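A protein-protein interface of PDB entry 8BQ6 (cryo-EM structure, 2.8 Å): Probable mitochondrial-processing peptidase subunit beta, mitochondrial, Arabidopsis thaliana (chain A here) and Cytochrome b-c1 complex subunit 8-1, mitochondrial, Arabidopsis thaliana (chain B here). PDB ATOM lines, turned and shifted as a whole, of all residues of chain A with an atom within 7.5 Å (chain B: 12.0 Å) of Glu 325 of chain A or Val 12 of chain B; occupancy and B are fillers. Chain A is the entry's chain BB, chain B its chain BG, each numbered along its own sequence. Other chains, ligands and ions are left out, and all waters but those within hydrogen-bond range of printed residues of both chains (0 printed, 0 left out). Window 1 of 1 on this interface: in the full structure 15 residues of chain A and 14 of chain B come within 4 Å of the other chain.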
ATOM      1  N   HIS A 236     -12.673  -6.137  29.525  1.00  0.00           N
ATOM      2  CA  HIS A 236     -12.272  -7.522  29.719  1.00  0.00           C
ATOM      3  C   HIS A 236     -10.757  -7.659  29.781  1.00  0.00           C
ATOM      4  O   HIS A 236     -10.248  -8.550  30.468  1.00  0.00           O
ATOM      5  CB  HIS A 236     -12.847  -8.403  28.610  1.00  0.00           C
ATOM      6  CG  HIS A 236     -14.309  -8.690  28.765  1.00  0.00           C
ATOM      7  ND1 HIS A 236     -14.783  -9.734  29.531  1.00  0.00           N
ATOM      8  CD2 HIS A 236     -15.400  -8.072  28.255  1.00  0.00           C
ATOM      9  CE1 HIS A 236     -16.104  -9.745  29.486  1.00  0.00           C
ATOM     10  NE2 HIS A 236     -16.502  -8.747  28.717  1.00  0.00           N
ATOM     11  N   LEU A 237     -10.020  -6.794  29.081  1.00  0.00           N
ATOM     12  CA  LEU A 237      -8.564  -6.868  29.146  1.00  0.00           C
ATOM     13  C   LEU A 237      -8.061  -6.551  30.548  1.00  0.00           C
ATOM     14  O   LEU A 237      -7.172  -7.236  31.065  1.00  0.00           O
ATOM     15  CB  LEU A 237      -7.938  -5.917  28.127  1.00  0.00           C
ATOM     16  CG  LEU A 237      -6.419  -6.037  28.018  1.00  0.00           C
ATOM     17  CD1 LEU A 237      -6.051  -7.305  27.275  1.00  0.00           C
ATOM     18  CD2 LEU A 237      -5.819  -4.822  27.335  1.00  0.00           C
ATOM     19  N   THR A 240      -8.864  -9.532  33.016  1.00  0.00           N
ATOM     20  CA  THR A 240      -8.014 -10.714  32.944  1.00  0.00           C
ATOM     21  C   THR A 240      -6.559 -10.384  33.270  1.00  0.00           C
ATOM     22  O   THR A 240      -5.886 -11.166  33.950  1.00  0.00           O
ATOM     23  CB  THR A 240      -8.150 -11.392  31.573  1.00  0.00           C
ATOM     24  OG1 THR A 240      -7.606 -12.714  31.638  1.00  0.00           O
ATOM     25  CG2 THR A 240      -7.441 -10.618  30.471  1.00  0.00           C
ATOM     26  N   ALA A 241      -6.058  -9.228  32.828  1.00  0.00           N
ATOM     27  CA  ALA A 241      -4.662  -8.899  33.096  1.00  0.00           C
ATOM     28  C   ALA A 241      -4.435  -8.617  34.573  1.00  0.00           C
ATOM     29  O   ALA A 241      -3.492  -9.143  35.176  1.00  0.00           O
ATOM     30  CB  ALA A 241      -4.226  -7.708  32.245  1.00  0.00           C
ATOM     31  N   GLN A 243      -6.280  -9.612  37.197  1.00  0.00           N
ATOM     32  CA  GLN A 243      -7.261 -10.415  37.908  1.00  0.00           C
ATOM     33  C   GLN A 243      -6.889 -10.500  39.378  1.00  0.00           C
ATOM     34  O   GLN A 243      -5.709 -10.475  39.741  1.00  0.00           O
ATOM     35  CB  GLN A 243      -7.363 -11.812  37.304  1.00  0.00           C
ATOM     36  CG  GLN A 243      -6.040 -12.483  37.057  1.00  0.00           C
ATOM     37  CD  GLN A 243      -6.205 -13.782  36.313  1.00  0.00           C
ATOM     38  OE1 GLN A 243      -5.910 -14.851  36.841  1.00  0.00           O
ATOM     39  NE2 GLN A 243      -6.682 -13.702  35.080  1.00  0.00           N
ATOM     40  N   THR A 322      -1.155 -10.709  35.326  1.00  0.00           N
ATOM     41  CA  THR A 322      -1.209 -12.151  35.111  1.00  0.00           C
ATOM     42  C   THR A 322      -1.411 -12.423  33.629  1.00  0.00           C
ATOM     43  O   THR A 322      -2.377 -11.938  33.032  1.00  0.00           O
ATOM     44  CB  THR A 322      -2.338 -12.797  35.916  1.00  0.00           C
ATOM     45  OG1 THR A 322      -2.091 -12.629  37.317  1.00  0.00           O
ATOM     46  CG2 THR A 322      -2.416 -14.276  35.611  1.00  0.00           C
ATOM     47  N   GLY A 323      -0.502 -13.197  33.039  1.00  0.00           N
ATOM     48  CA  GLY A 323      -0.677 -13.645  31.674  1.00  0.00           C
ATOM     49  C   GLY A 323      -1.893 -14.538  31.541  1.00  0.00           C
ATOM     50  O   GLY A 323      -1.984 -15.573  32.206  1.00  0.00           O
ATOM     51  N   SER A 324      -2.835 -14.145  30.691  1.00  0.00           N
ATOM     52  CA  SER A 324      -4.095 -14.859  30.544  1.00  0.00           C
ATOM     53  C   SER A 324      -4.797 -14.299  29.317  1.00  0.00           C
ATOM     54  O   SER A 324      -4.333 -13.336  28.699  1.00  0.00           O
ATOM     55  CB  SER A 324      -4.983 -14.718  31.780  1.00  0.00           C
ATOM     56  OG  SER A 324      -5.100 -13.360  32.163  1.00  0.00           O
ATOM     57  N   GLU A 325      -5.926 -14.908  28.971  1.00  0.00           N
ATOM     58  CA  GLU A 325      -6.719 -14.402  27.865  1.00  0.00           C
ATOM     59  C   GLU A 325      -8.186 -14.725  28.083  1.00  0.00           C
ATOM     60  O   GLU A 325      -8.537 -15.694  28.762  1.00  0.00           O
ATOM     61  CB  GLU A 325      -6.247 -14.977  26.530  1.00  0.00           C
ATOM     62  CG  GLU A 325      -7.001 -16.202  26.093  1.00  0.00           C
ATOM     63  CD  GLU A 325      -6.152 -17.095  25.241  1.00  0.00           C
ATOM     64  OE1 GLU A 325      -5.012 -16.691  24.941  1.00  0.00           O
ATOM     65  OE2 GLU A 325      -6.611 -18.198  24.884  1.00  0.00           O
ATOM     66  N   VAL A 326      -9.041 -13.892  27.497  1.00  0.00           N
ATOM     67  CA  VAL A 326     -10.476 -14.131  27.435  1.00  0.00           C
ATOM     68  C   VAL A 326     -10.920 -13.974  25.987  1.00  0.00           C
ATOM     69  O   VAL A 326     -10.648 -12.945  25.357  1.00  0.00           O
ATOM     70  CB  VAL A 326     -11.259 -13.188  28.372  1.00  0.00           C
ATOM     71  CG1 VAL A 326     -10.719 -11.771  28.300  1.00  0.00           C
ATOM     72  CG2 VAL A 326     -12.731 -13.205  28.026  1.00  0.00           C
ATOM     73  N   ARG A 327     -11.581 -15.002  25.457  1.00  0.00           N
ATOM     74  CA  ARG A 327     -12.050 -15.035  24.074  1.00  0.00           C
ATOM     75  C   ARG A 327     -13.569 -15.120  24.070  1.00  0.00           C
ATOM     76  O   ARG A 327     -14.138 -16.141  24.473  1.00  0.00           O
ATOM     77  CB  ARG A 327     -11.449 -16.217  23.314  1.00  0.00           C
ATOM     78  CG  ARG A 327     -10.060 -15.967  22.782  1.00  0.00           C
ATOM     79  CD  ARG A 327      -9.374 -17.259  22.389  1.00  0.00           C
ATOM     80  NE  ARG A 327      -7.926 -17.091  22.349  1.00  0.00           N
ATOM     81  CZ  ARG A 327      -7.231 -16.757  21.270  1.00  0.00           C
ATOM     82  NH1 ARG A 327      -7.812 -16.601  20.091  1.00  0.00           N
ATOM     83  NH2 ARG A 327      -5.919 -16.574  21.377  1.00  0.00           N
ATOM     84  N   MET A 328     -14.221 -14.060  23.597  1.00  0.00           N
ATOM     85  CA  MET A 328     -15.679 -14.004  23.478  1.00  0.00           C
ATOM     86  C   MET A 328     -16.037 -14.250  22.015  1.00  0.00           C
ATOM     87  O   MET A 328     -16.145 -13.320  21.217  1.00  0.00           O
ATOM     88  CB  MET A 328     -16.215 -12.666  23.974  1.00  0.00           C
ATOM     89  CG  MET A 328     -15.922 -12.375  25.438  1.00  0.00           C
ATOM     90  SD  MET A 328     -15.688 -10.627  25.820  1.00  0.00           S
ATOM     91  CE  MET A 328     -13.952 -10.401  25.447  1.00  0.00           C
ATOM     92  N   ILE A 329     -16.237 -15.516  21.667  1.00  0.00           N
ATOM     93  CA  ILE A 329     -16.434 -15.923  20.280  1.00  0.00           C
ATOM     94  C   ILE A 329     -17.886 -15.711  19.882  1.00  0.00           C
ATOM     95  O   ILE A 329     -18.798 -16.278  20.494  1.00  0.00           O
ATOM     96  CB  ILE A 329     -16.033 -17.387  20.069  1.00  0.00           C
ATOM     97  CG1 ILE A 329     -14.586 -17.610  20.488  1.00  0.00           C
ATOM     98  CG2 ILE A 329     -16.255 -17.784  18.622  1.00  0.00           C
ATOM     99  CD1 ILE A 329     -14.349 -18.974  21.061  1.00  0.00           C
ATOM    100  N   ILE A 505       1.717 -12.136  28.126  1.00  0.00           N
ATOM    101  CA  ILE A 505       0.817 -11.178  27.502  1.00  0.00           C
ATOM    102  C   ILE A 505      -0.606 -11.443  27.970  1.00  0.00           C
ATOM    103  O   ILE A 505      -0.929 -12.514  28.484  1.00  0.00           O
ATOM    104  CB  ILE A 505       0.923 -11.222  25.959  1.00  0.00           C
ATOM    105  CG1 ILE A 505       0.485 -12.580  25.413  1.00  0.00           C
ATOM    106  CG2 ILE A 505       2.343 -10.973  25.526  1.00  0.00           C
ATOM    107  CD1 ILE A 505      -0.853 -12.615  24.881  1.00  0.00           C
ATOM    108  N   ALA A 506      -1.454 -10.430  27.813  1.00  0.00           N
ATOM    109  CA  ALA A 506      -2.883 -10.546  28.067  1.00  0.00           C
ATOM    110  C   ALA A 506      -3.633 -10.303  26.767  1.00  0.00           C
ATOM    111  O   ALA A 506      -3.295  -9.386  26.015  1.00  0.00           O
ATOM    112  CB  ALA A 506      -3.347  -9.558  29.138  1.00  0.00           C
ATOM    113  N   ILE A 507      -4.646 -11.123  26.510  1.00  0.00           N
ATOM    114  CA  ILE A 507      -5.397 -11.091  25.263  1.00  0.00           C
ATOM    115  C   ILE A 507      -6.872 -10.951  25.590  1.00  0.00           C
ATOM    116  O   ILE A 507      -7.384 -11.646  26.473  1.00  0.00           O
ATOM    117  CB  ILE A 507      -5.149 -12.357  24.423  1.00  0.00           C
ATOM    118  CG1 ILE A 507      -3.757 -12.330  23.851  1.00  0.00           C
ATOM    119  CG2 ILE A 507      -6.155 -12.465  23.299  1.00  0.00           C
ATOM    120  CD1 ILE A 507      -3.416 -13.510  22.993  1.00  0.00           C
ATOM    121  N   SER A 508      -7.550 -10.046  24.889  1.00  0.00           N
ATOM    122  CA  SER A 508      -8.990  -9.861  25.010  1.00  0.00           C
ATOM    123  C   SER A 508      -9.577  -9.739  23.614  1.00  0.00           C
ATOM    124  O   SER A 508      -9.384  -8.717  22.952  1.00  0.00           O
ATOM    125  CB  SER A 508      -9.315  -8.615  25.833  1.00  0.00           C
ATOM    126  OG  SER A 508     -10.694  -8.553  26.136  1.00  0.00           O
ATOM    127  N   ALA A 509     -10.306 -10.762  23.173  1.00  0.00           N
ATOM    128  CA  ALA A 509     -10.823 -10.785  21.813  1.00  0.00           C
ATOM    129  C   ALA A 509     -12.317 -11.066  21.820  1.00  0.00           C
ATOM    130  O   ALA A 509     -12.824 -11.796  22.675  1.00  0.00           O
ATOM    131  CB  ALA A 509     -10.104 -11.833  20.956  1.00  0.00           C
ATOM    132  N   LEU A 516      -7.989 -16.406  15.092  1.00  0.00           N
ATOM    133  CA  LEU A 516      -6.983 -15.760  15.916  1.00  0.00           C
ATOM    134  C   LEU A 516      -6.060 -16.818  16.511  1.00  0.00           C
ATOM    135  O   LEU A 516      -6.541 -17.835  17.025  1.00  0.00           O
ATOM    136  CB  LEU A 516      -7.641 -14.931  17.015  1.00  0.00           C
ATOM    137  CG  LEU A 516      -6.790 -13.848  17.679  1.00  0.00           C
ATOM    138  CD1 LEU A 516      -6.573 -12.676  16.737  1.00  0.00           C
ATOM    139  CD2 LEU A 516      -7.444 -13.375  18.964  1.00  0.00           C
ATOM    140  N   PRO A 517      -4.744 -16.634  16.435  1.00  0.00           N
ATOM    141  CA  PRO A 517      -3.821 -17.616  17.012  1.00  0.00           C
ATOM    142  C   PRO A 517      -4.003 -17.728  18.514  1.00  0.00           C
ATOM    143  O   PRO A 517      -4.416 -16.780  19.184  1.00  0.00           O
ATOM    144  CB  PRO A 517      -2.442 -17.045  16.673  1.00  0.00           C
ATOM    145  CG  PRO A 517      -2.664 -16.193  15.496  1.00  0.00           C
ATOM    146  CD  PRO A 517      -4.045 -15.628  15.620  1.00  0.00           C
ATOM    147  N   ASP A 518      -3.680 -18.902  19.046  1.00  0.00           N
ATOM    148  CA  ASP A 518      -3.899 -19.151  20.461  1.00  0.00           C
ATOM    149  C   ASP A 518      -2.800 -18.509  21.306  1.00  0.00           C
ATOM    150  O   ASP A 518      -1.908 -17.817  20.806  1.00  0.00           O
ATOM    151  CB  ASP A 518      -4.017 -20.649  20.724  1.00  0.00           C
ATOM    152  CG  ASP A 518      -2.907 -21.450  20.085  1.00  0.00           C
ATOM    153  OD1 ASP A 518      -1.729 -21.049  20.172  1.00  0.00           O
ATOM    154  OD2 ASP A 518      -3.225 -22.488  19.476  1.00  0.00           O
ATOM    155  N   TYR A 519      -2.884 -18.739  22.621  1.00  0.00           N
ATOM    156  CA  TYR A 519      -1.981 -18.074  23.553  1.00  0.00           C
ATOM    157  C   TYR A 519      -0.534 -18.474  23.308  1.00  0.00           C
ATOM    158  O   TYR A 519       0.377 -17.651  23.449  1.00  0.00           O
ATOM    159  CB  TYR A 519      -2.377 -18.392  24.995  1.00  0.00           C
ATOM    160  CG  TYR A 519      -1.715 -17.474  25.987  1.00  0.00           C
ATOM    161  CD1 TYR A 519      -0.472 -17.774  26.522  1.00  0.00           C
ATOM    162  CD2 TYR A 519      -2.324 -16.293  26.369  1.00  0.00           C
ATOM    163  CE1 TYR A 519       0.136 -16.926  27.412  1.00  0.00           C
ATOM    164  CE2 TYR A 519      -1.730 -15.447  27.259  1.00  0.00           C
ATOM    165  CZ  TYR A 519      -0.501 -15.762  27.778  1.00  0.00           C
ATOM    166  OH  TYR A 519       0.090 -14.902  28.667  1.00  0.00           O
ATOM    167  N   ASN A 520      -0.302 -19.738  22.957  1.00  0.00           N
ATOM    168  CA  ASN A 520       1.066 -20.202  22.764  1.00  0.00           C
ATOM    169  C   ASN A 520       1.698 -19.569  21.532  1.00  0.00           C
ATOM    170  O   ASN A 520       2.914 -19.353  21.491  1.00  0.00           O
ATOM    171  CB  ASN A 520       1.092 -21.723  22.658  1.00  0.00           C
ATOM    172  CG  ASN A 520       1.006 -22.396  24.005  1.00  0.00           C
ATOM    173  OD1 ASN A 520       1.615 -21.943  24.971  1.00  0.00           O
ATOM    174  ND2 ASN A 520       0.265 -23.491  24.075  1.00  0.00           N
ATOM    175  N   PHE A 522       0.961 -16.450  20.282  1.00  0.00           N
ATOM    176  CA  PHE A 522       1.317 -15.095  20.693  1.00  0.00           C
ATOM    177  C   PHE A 522       2.502 -15.101  21.648  1.00  0.00           C
ATOM    178  O   PHE A 522       3.366 -14.220  21.588  1.00  0.00           O
ATOM    179  CB  PHE A 522       0.125 -14.416  21.359  1.00  0.00           C
ATOM    180  CG  PHE A 522      -0.877 -13.864  20.402  1.00  0.00           C
ATOM    181  CD1 PHE A 522      -0.735 -12.586  19.901  1.00  0.00           C
ATOM    182  CD2 PHE A 522      -1.979 -14.604  20.028  1.00  0.00           C
ATOM    183  CE1 PHE A 522      -1.659 -12.067  19.029  1.00  0.00           C
ATOM    184  CE2 PHE A 522      -2.907 -14.084  19.159  1.00  0.00           C
ATOM    185  CZ  PHE A 522      -2.747 -12.815  18.660  1.00  0.00           C
ATOM    186  N   LEU B   8     -20.105 -20.560  16.141  1.00  0.00           N
ATOM    187  CA  LEU B   8     -19.955 -20.981  17.526  1.00  0.00           C
ATOM    188  C   LEU B   8     -20.019 -19.762  18.437  1.00  0.00           C
ATOM    189  O   LEU B   8     -19.351 -18.754  18.191  1.00  0.00           O
ATOM    190  CB  LEU B   8     -18.628 -21.756  17.700  1.00  0.00           C
ATOM    191  CG  LEU B   8     -18.130 -22.372  19.018  1.00  0.00           C
ATOM    192  CD1 LEU B   8     -17.402 -21.405  19.941  1.00  0.00           C
ATOM    193  CD2 LEU B   8     -19.306 -23.007  19.737  1.00  0.00           C
ATOM    194  N   LYS B   9     -20.845 -19.845  19.476  1.00  0.00           N
ATOM    195  CA  LYS B   9     -20.946 -18.803  20.489  1.00  0.00           C
ATOM    196  C   LYS B   9     -20.459 -19.370  21.813  1.00  0.00           C
ATOM    197  O   LYS B   9     -21.055 -20.315  22.341  1.00  0.00           O
ATOM    198  CB  LYS B   9     -22.381 -18.284  20.611  1.00  0.00           C
ATOM    199  CG  LYS B   9     -22.547 -17.193  21.647  1.00  0.00           C
ATOM    200  CD  LYS B   9     -22.601 -15.825  21.009  1.00  0.00           C
ATOM    201  CE  LYS B   9     -23.105 -14.786  21.990  1.00  0.00           C
ATOM    202  NZ  LYS B   9     -24.487 -14.345  21.666  1.00  0.00           N
ATOM    203  N   ALA B  10     -19.376 -18.803  22.343  1.00  0.00           N
ATOM    204  CA  ALA B  10     -18.775 -19.302  23.571  1.00  0.00           C
ATOM    205  C   ALA B  10     -17.841 -18.247  24.140  1.00  0.00           C
ATOM    206  O   ALA B  10     -17.406 -17.333  23.438  1.00  0.00           O
ATOM    207  CB  ALA B  10     -18.006 -20.604  23.332  1.00  0.00           C
ATOM    208  N   VAL B  11     -17.534 -18.391  25.426  1.00  0.00           N
ATOM    209  CA  VAL B  11     -16.535 -17.573  26.099  1.00  0.00           C
ATOM    210  C   VAL B  11     -15.499 -18.504  26.707  1.00  0.00           C
ATOM    211  O   VAL B  11     -15.850 -19.454  27.417  1.00  0.00           O
ATOM    212  CB  VAL B  11     -17.160 -16.672  27.178  1.00  0.00           C
ATOM    213  CG1 VAL B  11     -16.085 -15.822  27.839  1.00  0.00           C
ATOM    214  CG2 VAL B  11     -18.241 -15.802  26.578  1.00  0.00           C
ATOM    215  N   VAL B  12     -14.227 -18.241  26.421  1.00  0.00           N
ATOM    216  CA  VAL B  12     -13.122 -19.067  26.890  1.00  0.00           C
ATOM    217  C   VAL B  12     -12.164 -18.185  27.673  1.00  0.00           C
ATOM    218  O   VAL B  12     -11.684 -17.170  27.157  1.00  0.00           O
ATOM    219  CB  VAL B  12     -12.388 -19.759  25.732  1.00  0.00           C
ATOM    220  CG1 VAL B  12     -11.423 -20.799  26.269  1.00  0.00           C
ATOM    221  CG2 VAL B  12     -13.372 -20.388  24.773  1.00  0.00           C
ATOM    222  N   TYR B  13     -11.880 -18.579  28.909  1.00  0.00           N
ATOM    223  CA  TYR B  13     -10.835 -17.967  29.715  1.00  0.00           C
ATOM    224  C   TYR B  13      -9.678 -18.946  29.829  1.00  0.00           C
ATOM    225  O   TYR B  13      -9.888 -20.121  30.145  1.00  0.00           O
ATOM    226  CB  TYR B  13     -11.338 -17.601  31.112  1.00  0.00           C
ATOM    227  CG  TYR B  13     -12.682 -16.921  31.163  1.00  0.00           C
ATOM    228  CD1 TYR B  13     -13.855 -17.652  31.059  1.00  0.00           C
ATOM    229  CD2 TYR B  13     -12.780 -15.553  31.352  1.00  0.00           C
ATOM    230  CE1 TYR B  13     -15.080 -17.041  31.116  1.00  0.00           C
ATOM    231  CE2 TYR B  13     -14.006 -14.931  31.414  1.00  0.00           C
ATOM    232  CZ  TYR B  13     -15.152 -15.682  31.297  1.00  0.00           C
ATOM    233  OH  TYR B  13     -16.382 -15.073  31.355  1.00  0.00           O
ATOM    234  N   ALA B  14      -8.464 -18.466  29.582  1.00  0.00           N
ATOM    235  CA  ALA B  14      -7.279 -19.303  29.638  1.00  0.00           C
ATOM    236  C   ALA B  14      -6.204 -18.623  30.471  1.00  0.00           C
ATOM    237  O   ALA B  14      -6.150 -17.395  30.564  1.00  0.00           O
ATOM    238  CB  ALA B  14      -6.742 -19.609  28.236  1.00  0.00           C
ATOM    239  N   LEU B  15      -5.345 -19.438  31.074  1.00  0.00           N
ATOM    240  CA  LEU B  15      -4.255 -18.970  31.916  1.00  0.00           C
ATOM    241  C   LEU B  15      -2.925 -19.318  31.261  1.00  0.00           C
ATOM    242  O   LEU B  15      -2.811 -20.336  30.573  1.00  0.00           O
ATOM    243  CB  LEU B  15      -4.345 -19.600  33.312  1.00  0.00           C
ATOM    244  CG  LEU B  15      -3.411 -19.108  34.420  1.00  0.00           C
ATOM    245  CD1 LEU B  15      -3.586 -17.625  34.658  1.00  0.00           C
ATOM    246  CD2 LEU B  15      -3.638 -19.885  35.705  1.00  0.00           C
ATOM    247  N   SER B  16      -1.927 -18.469  31.471  1.00  0.00           N
ATOM    248  CA  SER B  16      -0.614 -18.700  30.886  1.00  0.00           C
ATOM    249  C   SER B  16      -0.003 -19.992  31.428  1.00  0.00           C
ATOM    250  O   SER B  16      -0.144 -20.292  32.619  1.00  0.00           O
ATOM    251  CB  SER B  16       0.316 -17.526  31.188  1.00  0.00           C
ATOM    252  OG  SER B  16       1.623 -17.780  30.714  1.00  0.00           O
ATOM    253  N   PRO B  17       0.692 -20.767  30.592  1.00  0.00           N
ATOM    254  CA  PRO B  17       1.324 -22.002  31.088  1.00  0.00           C
ATOM    255  C   PRO B  17       2.363 -21.766  32.164  1.00  0.00           C
ATOM    256  O   PRO B  17       2.666 -22.692  32.924  1.00  0.00           O
ATOM    257  CB  PRO B  17       1.963 -22.608  29.831  1.00  0.00           C
ATOM    258  CG  PRO B  17       1.310 -21.933  28.687  1.00  0.00           C
ATOM    259  CD  PRO B  17       0.889 -20.582  29.146  1.00  0.00           C
ATOM    260  N   PHE B  18       2.921 -20.564  32.250  1.00  0.00           N
ATOM    261  CA  PHE B  18       3.937 -20.240  33.240  1.00  0.00           C
ATOM    262  C   PHE B  18       3.347 -19.700  34.534  1.00  0.00           C
ATOM    263  O   PHE B  18       4.103 -19.258  35.404  1.00  0.00           O
ATOM    264  CB  PHE B  18       4.928 -19.234  32.652  1.00  0.00           C
ATOM    265  CG  PHE B  18       5.524 -19.673  31.350  1.00  0.00           C
ATOM    266  CD1 PHE B  18       6.182 -20.885  31.252  1.00  0.00           C
ATOM    267  CD2 PHE B  18       5.411 -18.886  30.220  1.00  0.00           C
ATOM    268  CE1 PHE B  18       6.725 -21.298  30.057  1.00  0.00           C
ATOM    269  CE2 PHE B  18       5.952 -19.296  29.021  1.00  0.00           C
ATOM    270  CZ  PHE B  18       6.610 -20.503  28.941  1.00  0.00           C
ATOM    271  N   GLN B  19       2.022 -19.715  34.676  1.00  0.00           N
ATOM    272  CA  GLN B  19       1.354 -19.310  35.904  1.00  0.00           C
ATOM    273  C   GLN B  19       0.665 -20.469  36.608  1.00  0.00           C
ATOM    274  O   GLN B  19      -0.153 -20.236  37.503  1.00  0.00           O
ATOM    275  CB  GLN B  19       0.328 -18.213  35.624  1.00  0.00           C
ATOM    276  CG  GLN B  19       0.906 -16.900  35.165  1.00  0.00           C
ATOM    277  CD  GLN B  19       1.745 -16.237  36.228  1.00  0.00           C
ATOM    278  OE1 GLN B  19       2.812 -15.699  35.942  1.00  0.00           O
ATOM    279  NE2 GLN B  19       1.286 -16.299  37.470  1.00  0.00           N
ATOM    280  N   GLN B  20       0.954 -21.707  36.222  1.00  0.00           N
ATOM    281  CA  GLN B  20       0.334 -22.857  36.856  1.00  0.00           C
ATOM    282  C   GLN B  20       1.373 -23.947  37.045  1.00  0.00           C
ATOM    283  O   GLN B  20       2.406 -23.976  36.372  1.00  0.00           O
ATOM    284  CB  GLN B  20      -0.844 -23.395  36.040  1.00  0.00           C
ATOM    285  CG  GLN B  20      -0.703 -23.166  34.562  1.00  0.00           C
ATOM    286  CD  GLN B  20      -2.025 -23.229  33.850  1.00  0.00           C
ATOM    287  OE1 GLN B  20      -2.850 -24.095  34.130  1.00  0.00           O
ATOM    288  NE2 GLN B  20      -2.239 -22.310  32.923  1.00  0.00           N
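Among the printed residues, merely in contact across the chains: Ser 324 of chain A with Ala 14 of chain B (3.2 Å), Arg 327 of chain A with Val 11 of chain B (3.2 Å), Val 326 of chain A with Val 12 of chain B (3.3 Å), Ile 329 of chain A with Lys 9 of chain B (3.3 Å), Glu 325 of chain A with Tyr 13 of chain B (3.4 Å), Gly 323 of chain A with Leu 15 of chain B (3.6 Å), Arg 327 of chain A with Ala 10 of chain B (3.6 Å), Tyr 519 of chain A with Ser 16 of chain B (3.6 Å), Met 328 of chain A with Ala 10 of chain B (3.7 Å), Thr 322 of chain A with Leu 15 of chain B (3.7 Å), Asn 520 of chain A with Pro 17 of chain B (3.7 Å) and Glu 325 of chain A with Val 12 of chain B (3.8 Å).
No residue of chain B comes within 4 Å of Thr 240 of chain A. Gly 323 of chain A touches just these residues of chain B: Leu 15 and Ser 16. Glu 325 of chain A touches three residues of chain B. Of chain B, only Ala 10, Val 11 and Val 12 come within 4 Å of Arg 327 of chain A. Met 328 of chain A touches just one residue of chain B: Ala 10. Ile 329 of chain A touches just these residues of chain B: Leu 8 (3.3 Å), Lys 9 (3.3 Å) and Ala 10 (2.8 Å). No residue of chain B comes within 4 Å of Ala 506 of chain A. No residue of chain B comes within 4 Å of Ile 507 of chain A. No residue of chain B comes within 4 Å of Ser 508 of chain A. No residue of chain B comes within 4 Å of Asp 518 of chain A. Of the printed residues of chain A, Ala 10 of chain B touches Arg 327, Met 328 and Ile 329. Of the printed residues of chain A, Val 11 of chain B touches Arg 327 (3.2 Å). Val 12 of chain B touches three residues of chain A. Of the printed residues of chain A, Leu 15 of chain B touches Thr 322 (3.7 Å) and Gly 323 (3.6 Å). Printed residues of chain A within 4 Å of Ser 16 of chain B: Gly 323 (3.0 Å) and Tyr 519 (3.6 Å). The nearest residue of chain B that does not touch Glu 325 of chain A is Leu 15 of chain B (5.0 Å). The nearest residue of chain A that does not touch Val 12 of chain B is Ile 329 of chain A (4.1 Å).
N of Ser 324 of chain A lies within hydrogen-bond range of O of Ile 505 of chain A (3.3 Å). The backbone carbonyl oxygen of Ser 324 of chain A sits at hydrogen-bond distance from the backbone NH of Ile 507 of chain A, 3.1 Å away. N of Val 326 of chain A is in hydrogen-bond range of O of Ile 507 of chain A (3.0 Å). NH2 of Arg 327 of chain A lies within hydrogen-bond range of O of Pro 517 of chain A, at 2.7 Å. O of Ala 509 of chain A is in hydrogen-bond range of N of Met 328 of chain A (2.8 Å). NE2 of Gln 20 of chain B sits at hydrogen-bond distance from O of Leu 15 of chain B (3.1 Å).
The backbone NH of Ser 16 of chain B sits at hydrogen-bond distance from the backbone carbonyl oxygen of Gly 323 of chain A. N of Ala 14 of chain B is in hydrogen-bond range of O of Glu 325 of chain A (2.9 Å). The backbone carbonyl oxygen (O) of Val 12 of chain B lies within hydrogen-bond range of the backbone NH (N) of Arg 327 of chain A (2.8 Å). N of Ile 329 of chain A is in hydrogen-bond range of O of Ala 10 of chain B, 2.8 Å away. The backbone carbonyl oxygen (O) of Ile 329 of chain A lies close to the backbone carbonyl oxygen (O) of Leu 8 of chain B, at 3.4 Å.
Hydrophobic or aromatic side chains of chain B that line the printed part of chain A: Val 11, Ala 14, Leu 15 and Pro 17. Among the printed residues, no Asp or Glu carboxylate lies within 4 Å of a Lys or Arg side-chain nitrogen of the other chain.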
